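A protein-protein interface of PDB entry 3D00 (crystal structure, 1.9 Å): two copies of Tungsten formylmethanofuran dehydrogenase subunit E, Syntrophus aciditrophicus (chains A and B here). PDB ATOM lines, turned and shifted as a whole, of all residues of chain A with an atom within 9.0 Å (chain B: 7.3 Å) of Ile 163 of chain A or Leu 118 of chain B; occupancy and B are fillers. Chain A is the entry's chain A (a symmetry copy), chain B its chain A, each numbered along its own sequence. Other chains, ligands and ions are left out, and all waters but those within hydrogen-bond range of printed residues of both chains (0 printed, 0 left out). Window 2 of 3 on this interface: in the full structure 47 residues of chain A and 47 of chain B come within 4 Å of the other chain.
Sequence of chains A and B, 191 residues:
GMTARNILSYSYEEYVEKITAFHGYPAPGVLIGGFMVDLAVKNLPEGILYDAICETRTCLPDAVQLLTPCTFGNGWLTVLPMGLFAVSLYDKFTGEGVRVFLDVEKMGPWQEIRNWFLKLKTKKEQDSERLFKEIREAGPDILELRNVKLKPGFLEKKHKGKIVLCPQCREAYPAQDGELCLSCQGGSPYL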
ATOM      1  N   HIS A 159      18.757 -23.936   5.922  1.00  0.00           N
ATOM      2  CA  HIS A 159      17.803 -23.525   6.989  1.00  0.00           C
ATOM      3  C   HIS A 159      18.491 -23.353   8.336  1.00  0.00           C
ATOM      4  O   HIS A 159      19.254 -24.229   8.753  1.00  0.00           O
ATOM      5  CB  HIS A 159      16.660 -24.552   7.127  1.00  0.00           C
ATOM      6  N   LYS A 160      18.201 -22.236   9.012  1.00  0.00           N
ATOM      7  CA  LYS A 160      18.800 -21.919  10.325  1.00  0.00           C
ATOM      8  C   LYS A 160      18.219 -22.772  11.465  1.00  0.00           C
ATOM      9  O   LYS A 160      17.620 -22.211  12.380  1.00  0.00           O
ATOM     10  CB  LYS A 160      18.573 -20.439  10.668  1.00  0.00           C
ATOM     11  N   GLY A 161      18.420 -24.099  11.421  1.00  0.00           N
ATOM     12  CA  GLY A 161      17.750 -25.067  12.326  1.00  0.00           C
ATOM     13  C   GLY A 161      17.939 -24.890  13.832  1.00  0.00           C
ATOM     14  O   GLY A 161      19.003 -24.474  14.295  1.00  0.00           O
ATOM     15  N   LYS A 162      16.886 -25.190  14.589  1.00  0.00           N
ATOM     16  CA  LYS A 162      16.923 -25.202  16.052  1.00  0.00           C
ATOM     17  C   LYS A 162      17.436 -26.577  16.538  1.00  0.00           C
ATOM     18  O   LYS A 162      16.978 -27.619  16.048  1.00  0.00           O
ATOM     19  CB  LYS A 162      15.521 -24.905  16.610  1.00  0.00           C
ATOM     20  CG  LYS A 162      15.461 -24.647  18.108  1.00  0.00           C
ATOM     21  CD  LYS A 162      14.032 -24.377  18.598  1.00  0.00           C
ATOM     22  N   ILE A 163      18.391 -26.575  17.472  1.00  0.00           N
ATOM     23  CA  ILE A 163      18.998 -27.808  17.999  1.00  0.00           C
ATOM     24  C   ILE A 163      18.300 -28.253  19.275  1.00  0.00           C
ATOM     25  O   ILE A 163      18.227 -27.501  20.223  1.00  0.00           O
ATOM     26  CB  ILE A 163      20.533 -27.627  18.281  1.00  0.00           C
ATOM     27  CG1 ILE A 163      21.256 -27.262  16.993  1.00  0.00           C
ATOM     28  CG2 ILE A 163      21.166 -28.910  18.874  1.00  0.00           C
ATOM     29  CD1 ILE A 163      21.080 -28.267  15.890  1.00  0.00           C
ATOM     30  N   VAL A 164      17.775 -29.471  19.285  1.00  0.00           N
ATOM     31  CA  VAL A 164      17.126 -30.033  20.469  1.00  0.00           C
ATOM     32  C   VAL A 164      17.843 -31.319  20.918  1.00  0.00           C
ATOM     33  O   VAL A 164      18.815 -31.735  20.271  1.00  0.00           O
ATOM     34  CB  VAL A 164      15.632 -30.313  20.181  1.00  0.00           C
ATOM     35  CG1 VAL A 164      14.869 -29.004  20.075  1.00  0.00           C
ATOM     36  CG2 VAL A 164      15.469 -31.145  18.898  1.00  0.00           C
ATOM     37  N   LEU A 165      17.368 -31.929  22.010  1.00  0.00           N
ATOM     38  CA  LEU A 165      17.959 -33.159  22.582  1.00  0.00           C
ATOM     39  C   LEU A 165      17.079 -34.391  22.347  1.00  0.00           C
ATOM     40  O   LEU A 165      15.920 -34.426  22.760  1.00  0.00           O
ATOM     41  CB  LEU A 165      18.202 -33.003  24.092  1.00  0.00           C
ATOM     42  CG  LEU A 165      19.007 -34.085  24.833  1.00  0.00           C
ATOM     43  CD1 LEU A 165      20.384 -34.236  24.212  1.00  0.00           C
ATOM     44  CD2 LEU A 165      19.113 -33.847  26.357  1.00  0.00           C
ATOM     45  N   CYS A 166      17.631 -35.418  21.711  1.00  0.00           N
ATOM     46  CA  CYS A 166      16.850 -36.633  21.462  1.00  0.00           C
ATOM     47  C   CYS A 166      16.605 -37.322  22.778  1.00  0.00           C
ATOM     48  O   CYS A 166      17.551 -37.606  23.493  1.00  0.00           O
ATOM     49  CB  CYS A 166      17.578 -37.568  20.522  1.00  0.00           C
ATOM     50  SG  CYS A 166      16.643 -39.073  20.212  1.00  0.00           S
ATOM     51  N   GLU A 171      21.405 -37.189  22.400  1.00  0.00           N
ATOM     52  CA  GLU A 171      22.320 -36.429  21.585  1.00  0.00           C
ATOM     53  C   GLU A 171      21.590 -35.248  20.948  1.00  0.00           C
ATOM     54  O   GLU A 171      20.378 -35.285  20.763  1.00  0.00           O
ATOM     55  CB  GLU A 171      22.973 -37.343  20.544  1.00  0.00           C
ATOM     56  CG  GLU A 171      24.139 -38.157  21.144  1.00  0.00           C
ATOM     57  CD  GLU A 171      24.683 -39.212  20.225  1.00  0.00           C
ATOM     58  OE1 GLU A 171      25.112 -38.844  19.101  1.00  0.00           O
ATOM     59  OE2 GLU A 171      24.686 -40.406  20.626  1.00  0.00           O
ATOM     60  N   ALA A 172      22.333 -34.201  20.632  1.00  0.00           N
ATOM     61  CA  ALA A 172      21.779 -33.041  19.965  1.00  0.00           C
ATOM     62  C   ALA A 172      21.511 -33.336  18.475  1.00  0.00           C
ATOM     63  O   ALA A 172      22.278 -34.022  17.794  1.00  0.00           O
ATOM     64  CB  ALA A 172      22.692 -31.834  20.121  1.00  0.00           C
ATOM     65  N   TYR A 173      20.374 -32.834  18.001  1.00  0.00           N
ATOM     66  CA  TYR A 173      19.951 -32.993  16.617  1.00  0.00           C
ATOM     67  C   TYR A 173      19.017 -31.819  16.202  1.00  0.00           C
ATOM     68  O   TYR A 173      18.509 -31.101  17.051  1.00  0.00           O
ATOM     69  CB  TYR A 173      19.296 -34.382  16.403  1.00  0.00           C
ATOM     70  CG  TYR A 173      17.897 -34.479  16.919  1.00  0.00           C
ATOM     71  CD1 TYR A 173      17.639 -34.568  18.278  1.00  0.00           C
ATOM     72  CD2 TYR A 173      16.811 -34.426  16.056  1.00  0.00           C
ATOM     73  CE1 TYR A 173      16.327 -34.610  18.773  1.00  0.00           C
ATOM     74  CE2 TYR A 173      15.488 -34.481  16.555  1.00  0.00           C
ATOM     75  CZ  TYR A 173      15.261 -34.581  17.911  1.00  0.00           C
ATOM     76  OH  TYR A 173      13.964 -34.636  18.435  1.00  0.00           O
ATOM     77  N   PRO A 174      18.839 -31.599  14.890  1.00  0.00           N
ATOM     78  CA  PRO A 174      17.875 -30.620  14.375  1.00  0.00           C
ATOM     79  C   PRO A 174      16.419 -30.996  14.693  1.00  0.00           C
ATOM     80  O   PRO A 174      15.987 -32.123  14.409  1.00  0.00           O
ATOM     81  CB  PRO A 174      18.102 -30.667  12.868  1.00  0.00           C
ATOM     82  CG  PRO A 174      19.416 -31.347  12.669  1.00  0.00           C
ATOM     83  CD  PRO A 174      19.579 -32.269  13.803  1.00  0.00           C
ATOM     84  N   ALA A 175      15.681 -30.054  15.289  1.00  0.00           N
ATOM     85  CA  ALA A 175      14.282 -30.274  15.703  1.00  0.00           C
ATOM     86  C   ALA A 175      13.356 -30.642  14.542  1.00  0.00           C
ATOM     87  O   ALA A 175      12.338 -31.329  14.733  1.00  0.00           O
ATOM     88  CB  ALA A 175      13.743 -29.042  16.412  1.00  0.00           C
ATOM     89  N   GLN A 176      13.719 -30.195  13.347  1.00  0.00           N
ATOM     90  CA  GLN A 176      12.927 -30.486  12.164  1.00  0.00           C
ATOM     91  C   GLN A 176      12.867 -31.983  11.868  1.00  0.00           C
ATOM     92  O   GLN A 176      11.901 -32.460  11.296  1.00  0.00           O
ATOM     93  CB  GLN A 176      13.451 -29.699  10.955  1.00  0.00           C
ATOM     94  CG  GLN A 176      14.729 -30.230  10.386  1.00  0.00           C
ATOM     95  CD  GLN A 176      15.770 -29.152  10.066  1.00  0.00           C
ATOM     96  OE1 GLN A 176      15.723 -28.029  10.599  1.00  0.00           O
ATOM     97  NE2 GLN A 176      16.744 -29.510   9.227  1.00  0.00           N
ATOM     98  N   ASP A 177      13.880 -32.727  12.286  1.00  0.00           N
ATOM     99  CA  ASP A 177      13.945 -34.147  11.964  1.00  0.00           C
ATOM    100  C   ASP A 177      12.861 -34.984  12.655  1.00  0.00           C
ATOM    101  O   ASP A 177      12.640 -36.135  12.257  1.00  0.00           O
ATOM    102  CB  ASP A 177      15.338 -34.728  12.310  1.00  0.00           C
ATOM    103  CG  ASP A 177      16.445 -34.189  11.440  1.00  0.00           C
ATOM    104  OD1 ASP A 177      16.134 -33.507  10.464  1.00  0.00           O
ATOM    105  OD2 ASP A 177      17.641 -34.433  11.739  1.00  0.00           O
ATOM    106  N   GLY B  83      22.398 -35.674  10.919  1.00  0.00           N
ATOM    107  CA  GLY B  83      22.537 -34.472  11.743  1.00  0.00           C
ATOM    108  C   GLY B  83      23.152 -34.675  13.112  1.00  0.00           C
ATOM    109  O   GLY B  83      23.071 -33.795  13.958  1.00  0.00           O
ATOM    110  N   VAL B 104      27.657 -33.211  25.880  1.00  0.00           N
ATOM    111  CA  VAL B 104      27.337 -31.859  26.398  1.00  0.00           C
ATOM    112  C   VAL B 104      27.412 -31.792  27.928  1.00  0.00           C
ATOM    113  O   VAL B 104      27.760 -30.728  28.472  1.00  0.00           O
ATOM    114  CB  VAL B 104      25.993 -31.320  25.855  1.00  0.00           C
ATOM    115  CG1 VAL B 104      25.700 -29.900  26.404  1.00  0.00           C
ATOM    116  CG2 VAL B 104      26.024 -31.309  24.325  1.00  0.00           C
ATOM    117  N   MET B 107      30.602 -30.241  28.758  1.00  0.00           N
ATOM    118  CA  MET B 107      30.864 -28.844  28.369  1.00  0.00           C
ATOM    119  C   MET B 107      30.279 -27.857  29.380  1.00  0.00           C
ATOM    120  O   MET B 107      29.311 -27.108  29.075  1.00  0.00           O
ATOM    121  CB  MET B 107      30.259 -28.521  27.016  1.00  0.00           C
ATOM    122  CG  MET B 107      30.596 -29.451  25.912  1.00  0.00           C
ATOM    123  SD  MET B 107      29.478 -28.917  24.513  1.00  0.00           S
ATOM    124  CE  MET B 107      29.503 -30.593  23.610  1.00  0.00           C
ATOM    125  N   GLU B 112      31.556 -21.484  25.166  1.00  0.00           N
ATOM    126  CA  GLU B 112      31.711 -21.169  23.736  1.00  0.00           C
ATOM    127  C   GLU B 112      31.518 -22.389  22.858  1.00  0.00           C
ATOM    128  O   GLU B 112      30.815 -22.318  21.864  1.00  0.00           O
ATOM    129  CB  GLU B 112      33.061 -20.508  23.430  1.00  0.00           C
ATOM    130  CG  GLU B 112      33.132 -19.006  23.779  1.00  0.00           C
ATOM    131  CD  GLU B 112      32.091 -18.168  23.031  1.00  0.00           C
ATOM    132  OE1 GLU B 112      31.995 -18.270  21.783  1.00  0.00           O
ATOM    133  OE2 GLU B 112      31.366 -17.403  23.698  1.00  0.00           O
ATOM    134  N   ILE B 113      32.131 -23.509  23.226  1.00  0.00           N
ATOM    135  CA  ILE B 113      31.847 -24.754  22.536  1.00  0.00           C
ATOM    136  C   ILE B 113      30.350 -25.070  22.641  1.00  0.00           C
ATOM    137  O   ILE B 113      29.725 -25.441  21.656  1.00  0.00           O
ATOM    138  CB  ILE B 113      32.683 -25.909  23.050  1.00  0.00           C
ATOM    139  CG1 ILE B 113      34.176 -25.608  22.901  1.00  0.00           C
ATOM    140  CG2 ILE B 113      32.323 -27.188  22.277  1.00  0.00           C
ATOM    141  CD1 ILE B 113      35.055 -26.754  23.374  1.00  0.00           C
ATOM    142  N   ARG B 114      29.743 -24.865  23.806  1.00  0.00           N
ATOM    143  CA  ARG B 114      28.333 -25.189  23.965  1.00  0.00           C
ATOM    144  C   ARG B 114      27.465 -24.302  23.102  1.00  0.00           C
ATOM    145  O   ARG B 114      26.518 -24.774  22.489  1.00  0.00           O
ATOM    146  CB  ARG B 114      27.917 -25.078  25.419  1.00  0.00           C
ATOM    147  CG  ARG B 114      26.509 -25.604  25.726  1.00  0.00           C
ATOM    148  CD  ARG B 114      26.251 -25.728  27.295  1.00  0.00           C
ATOM    149  NE  ARG B 114      26.250 -24.442  27.997  1.00  0.00           N
ATOM    150  CZ  ARG B 114      25.326 -23.487  27.841  1.00  0.00           C
ATOM    151  NH1 ARG B 114      24.307 -23.656  26.981  1.00  0.00           N
ATOM    152  NH2 ARG B 114      25.419 -22.341  28.535  1.00  0.00           N
ATOM    153  N   ASN B 115      27.792 -23.015  23.031  1.00  0.00           N
ATOM    154  CA  ASN B 115      26.991 -22.069  22.256  1.00  0.00           C
ATOM    155  C   ASN B 115      27.065 -22.411  20.781  1.00  0.00           C
ATOM    156  O   ASN B 115      26.072 -22.335  20.073  1.00  0.00           O
ATOM    157  CB  ASN B 115      27.431 -20.609  22.493  1.00  0.00           C
ATOM    158  CG  ASN B 115      27.062 -20.074  23.903  1.00  0.00           C
ATOM    159  OD1 ASN B 115      26.199 -20.628  24.602  1.00  0.00           O
ATOM    160  ND2 ASN B 115      27.742 -19.003  24.322  1.00  0.00           N
ATOM    161  N   TRP B 116      28.260 -22.797  20.337  1.00  0.00           N
ATOM    162  CA  TRP B 116      28.497 -23.300  18.974  1.00  0.00           C
ATOM    163  C   TRP B 116      27.725 -24.603  18.714  1.00  0.00           C
ATOM    164  O   TRP B 116      27.008 -24.727  17.726  1.00  0.00           O
ATOM    165  CB  TRP B 116      30.010 -23.539  18.730  1.00  0.00           C
ATOM    166  CG  TRP B 116      30.266 -24.323  17.457  1.00  0.00           C
ATOM    167  CD1 TRP B 116      30.282 -23.835  16.183  1.00  0.00           C
ATOM    168  CD2 TRP B 116      30.469 -25.731  17.345  1.00  0.00           C
ATOM    169  NE1 TRP B 116      30.492 -24.841  15.285  1.00  0.00           N
ATOM    170  CE2 TRP B 116      30.610 -26.023  15.963  1.00  0.00           C
ATOM    171  CE3 TRP B 116      30.550 -26.782  18.274  1.00  0.00           C
ATOM    172  CZ2 TRP B 116      30.843 -27.299  15.494  1.00  0.00           C
ATOM    173  CZ3 TRP B 116      30.774 -28.060  17.812  1.00  0.00           C
ATOM    174  CH2 TRP B 116      30.909 -28.315  16.417  1.00  0.00           C
ATOM    175  N   PHE B 117      27.892 -25.574  19.610  1.00  0.00           N
ATOM    176  CA  PHE B 117      27.292 -26.886  19.411  1.00  0.00           C
ATOM    177  C   PHE B 117      25.782 -26.747  19.350  1.00  0.00           C
ATOM    178  O   PHE B 117      25.164 -27.308  18.479  1.00  0.00           O
ATOM    179  CB  PHE B 117      27.740 -27.878  20.505  1.00  0.00           C
ATOM    180  CG  PHE B 117      27.283 -29.300  20.273  1.00  0.00           C
ATOM    181  CD1 PHE B 117      27.581 -29.962  19.090  1.00  0.00           C
ATOM    182  CD2 PHE B 117      26.569 -29.983  21.237  1.00  0.00           C
ATOM    183  CE1 PHE B 117      27.164 -31.273  18.879  1.00  0.00           C
ATOM    184  CE2 PHE B 117      26.157 -31.287  21.023  1.00  0.00           C
ATOM    185  CZ  PHE B 117      26.450 -31.925  19.832  1.00  0.00           C
ATOM    186  N   LEU B 118      25.206 -25.938  20.228  1.00  0.00           N
ATOM    187  CA  LEU B 118      23.746 -25.797  20.324  1.00  0.00           C
ATOM    188  C   LEU B 118      23.216 -24.640  19.493  1.00  0.00           C
ATOM    189  O   LEU B 118      22.018 -24.347  19.518  1.00  0.00           O
ATOM    190  CB  LEU B 118      23.330 -25.619  21.786  1.00  0.00           C
ATOM    191  CG  LEU B 118      23.945 -26.620  22.762  1.00  0.00           C
ATOM    192  CD1 LEU B 118      23.496 -26.292  24.182  1.00  0.00           C
ATOM    193  CD2 LEU B 118      23.617 -28.059  22.379  1.00  0.00           C
ATOM    194  N   LYS B 119      24.107 -23.984  18.745  1.00  0.00           N
ATOM    195  CA  LYS B 119      23.739 -22.818  17.925  1.00  0.00           C
ATOM    196  C   LYS B 119      22.975 -21.708  18.717  1.00  0.00           C
ATOM    197  O   LYS B 119      22.105 -21.037  18.178  1.00  0.00           O
ATOM    198  CB  LYS B 119      22.959 -23.279  16.681  1.00  0.00           C
ATOM    199  CG  LYS B 119      23.704 -24.316  15.851  1.00  0.00           C
ATOM    200  CD  LYS B 119      22.932 -24.819  14.636  1.00  0.00           C
ATOM    201  N   LEU B 120      23.330 -21.505  19.988  1.00  0.00           N
ATOM    202  CA  LEU B 120      22.692 -20.480  20.816  1.00  0.00           C
ATOM    203  C   LEU B 120      23.175 -19.088  20.399  1.00  0.00           C
ATOM    204  O   LEU B 120      24.386 -18.891  20.247  1.00  0.00           O
ATOM    205  CB  LEU B 120      23.025 -20.678  22.305  1.00  0.00           C
ATOM    206  CG  LEU B 120      22.817 -22.055  22.932  1.00  0.00           C
ATOM    207  CD1 LEU B 120      23.132 -22.051  24.429  1.00  0.00           C
ATOM    208  CD2 LEU B 120      21.410 -22.544  22.668  1.00  0.00           C
ATOM    209  N   LYS B 121      22.232 -18.136  20.252  1.00  0.00           N
ATOM    210  CA  LYS B 121      22.514 -16.713  19.877  1.00  0.00           C
ATOM    211  C   LYS B 121      21.849 -15.720  20.833  1.00  0.00           C
ATOM    212  O   LYS B 121      21.574 -16.039  21.985  1.00  0.00           O
ATOM    213  CB  LYS B 121      22.065 -16.406  18.427  1.00  0.00           C
ATOM    214  CG  LYS B 121      22.612 -17.368  17.366  1.00  0.00           C
ATOM    215  CD  LYS B 121      22.160 -17.002  15.943  1.00  0.00           C
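Gly 161 of chain A touches Lys 119 of chain B. Ile 163 of chain A touches Leu 118 of chain B. CG1 of Ile 163 of chain A touches CD of Lys 119 of chain B, at 3.8 Å. O of Gly 83 of chain B touches O of Ala 172 of chain A, 3.9 Å away. Ala 172 of chain A touches Phe 117 of chain B (CB to CE2, 3.6 Å). Gly 83 of chain B touches Pro 174 of chain A (O to CD, 3.8 Å).
Printed residues of chain B within 4 Å of Ile 163 of chain A: Leu 118 and Lys 119. Of the printed residues of chain A, Leu 118 of chain B touches Ile 163. Printed residues of chain A within 4 Å of Lys 119 of chain B: Gly 161 and Ile 163. Printed residues of chain B within 4 Å of Pro 174 of chain A: Gly 83. Printed residues of chain A within 4 Å of Phe 117 of chain B: Ala 172. Of the printed residues of chain A, Gly 83 of chain B touches Ala 172 and Pro 174. Printed residues of chain B within 4 Å of Ala 172 of chain A: Gly 83 and Phe 117. The nearest printed residue of chain B that does not touch Ile 163 of chain A is Phe 117 of chain B (4.2 Å). The nearest printed residue of chain B that does not touch Gly 161 of chain A is Leu 118 of chain B (6.0 Å).
Hydrophobic or aromatic side chains of chain A that line the printed part of chain B: Ile 163, Ala 172 and Pro 174. Among the printed residues, 6 pairs touch across the chains. Among the printed residues, no Asp or Glu carboxylate lies within 4 Å of a Lys or Arg side-chain nitrogen of the other chain.
No position is printed for both chains.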
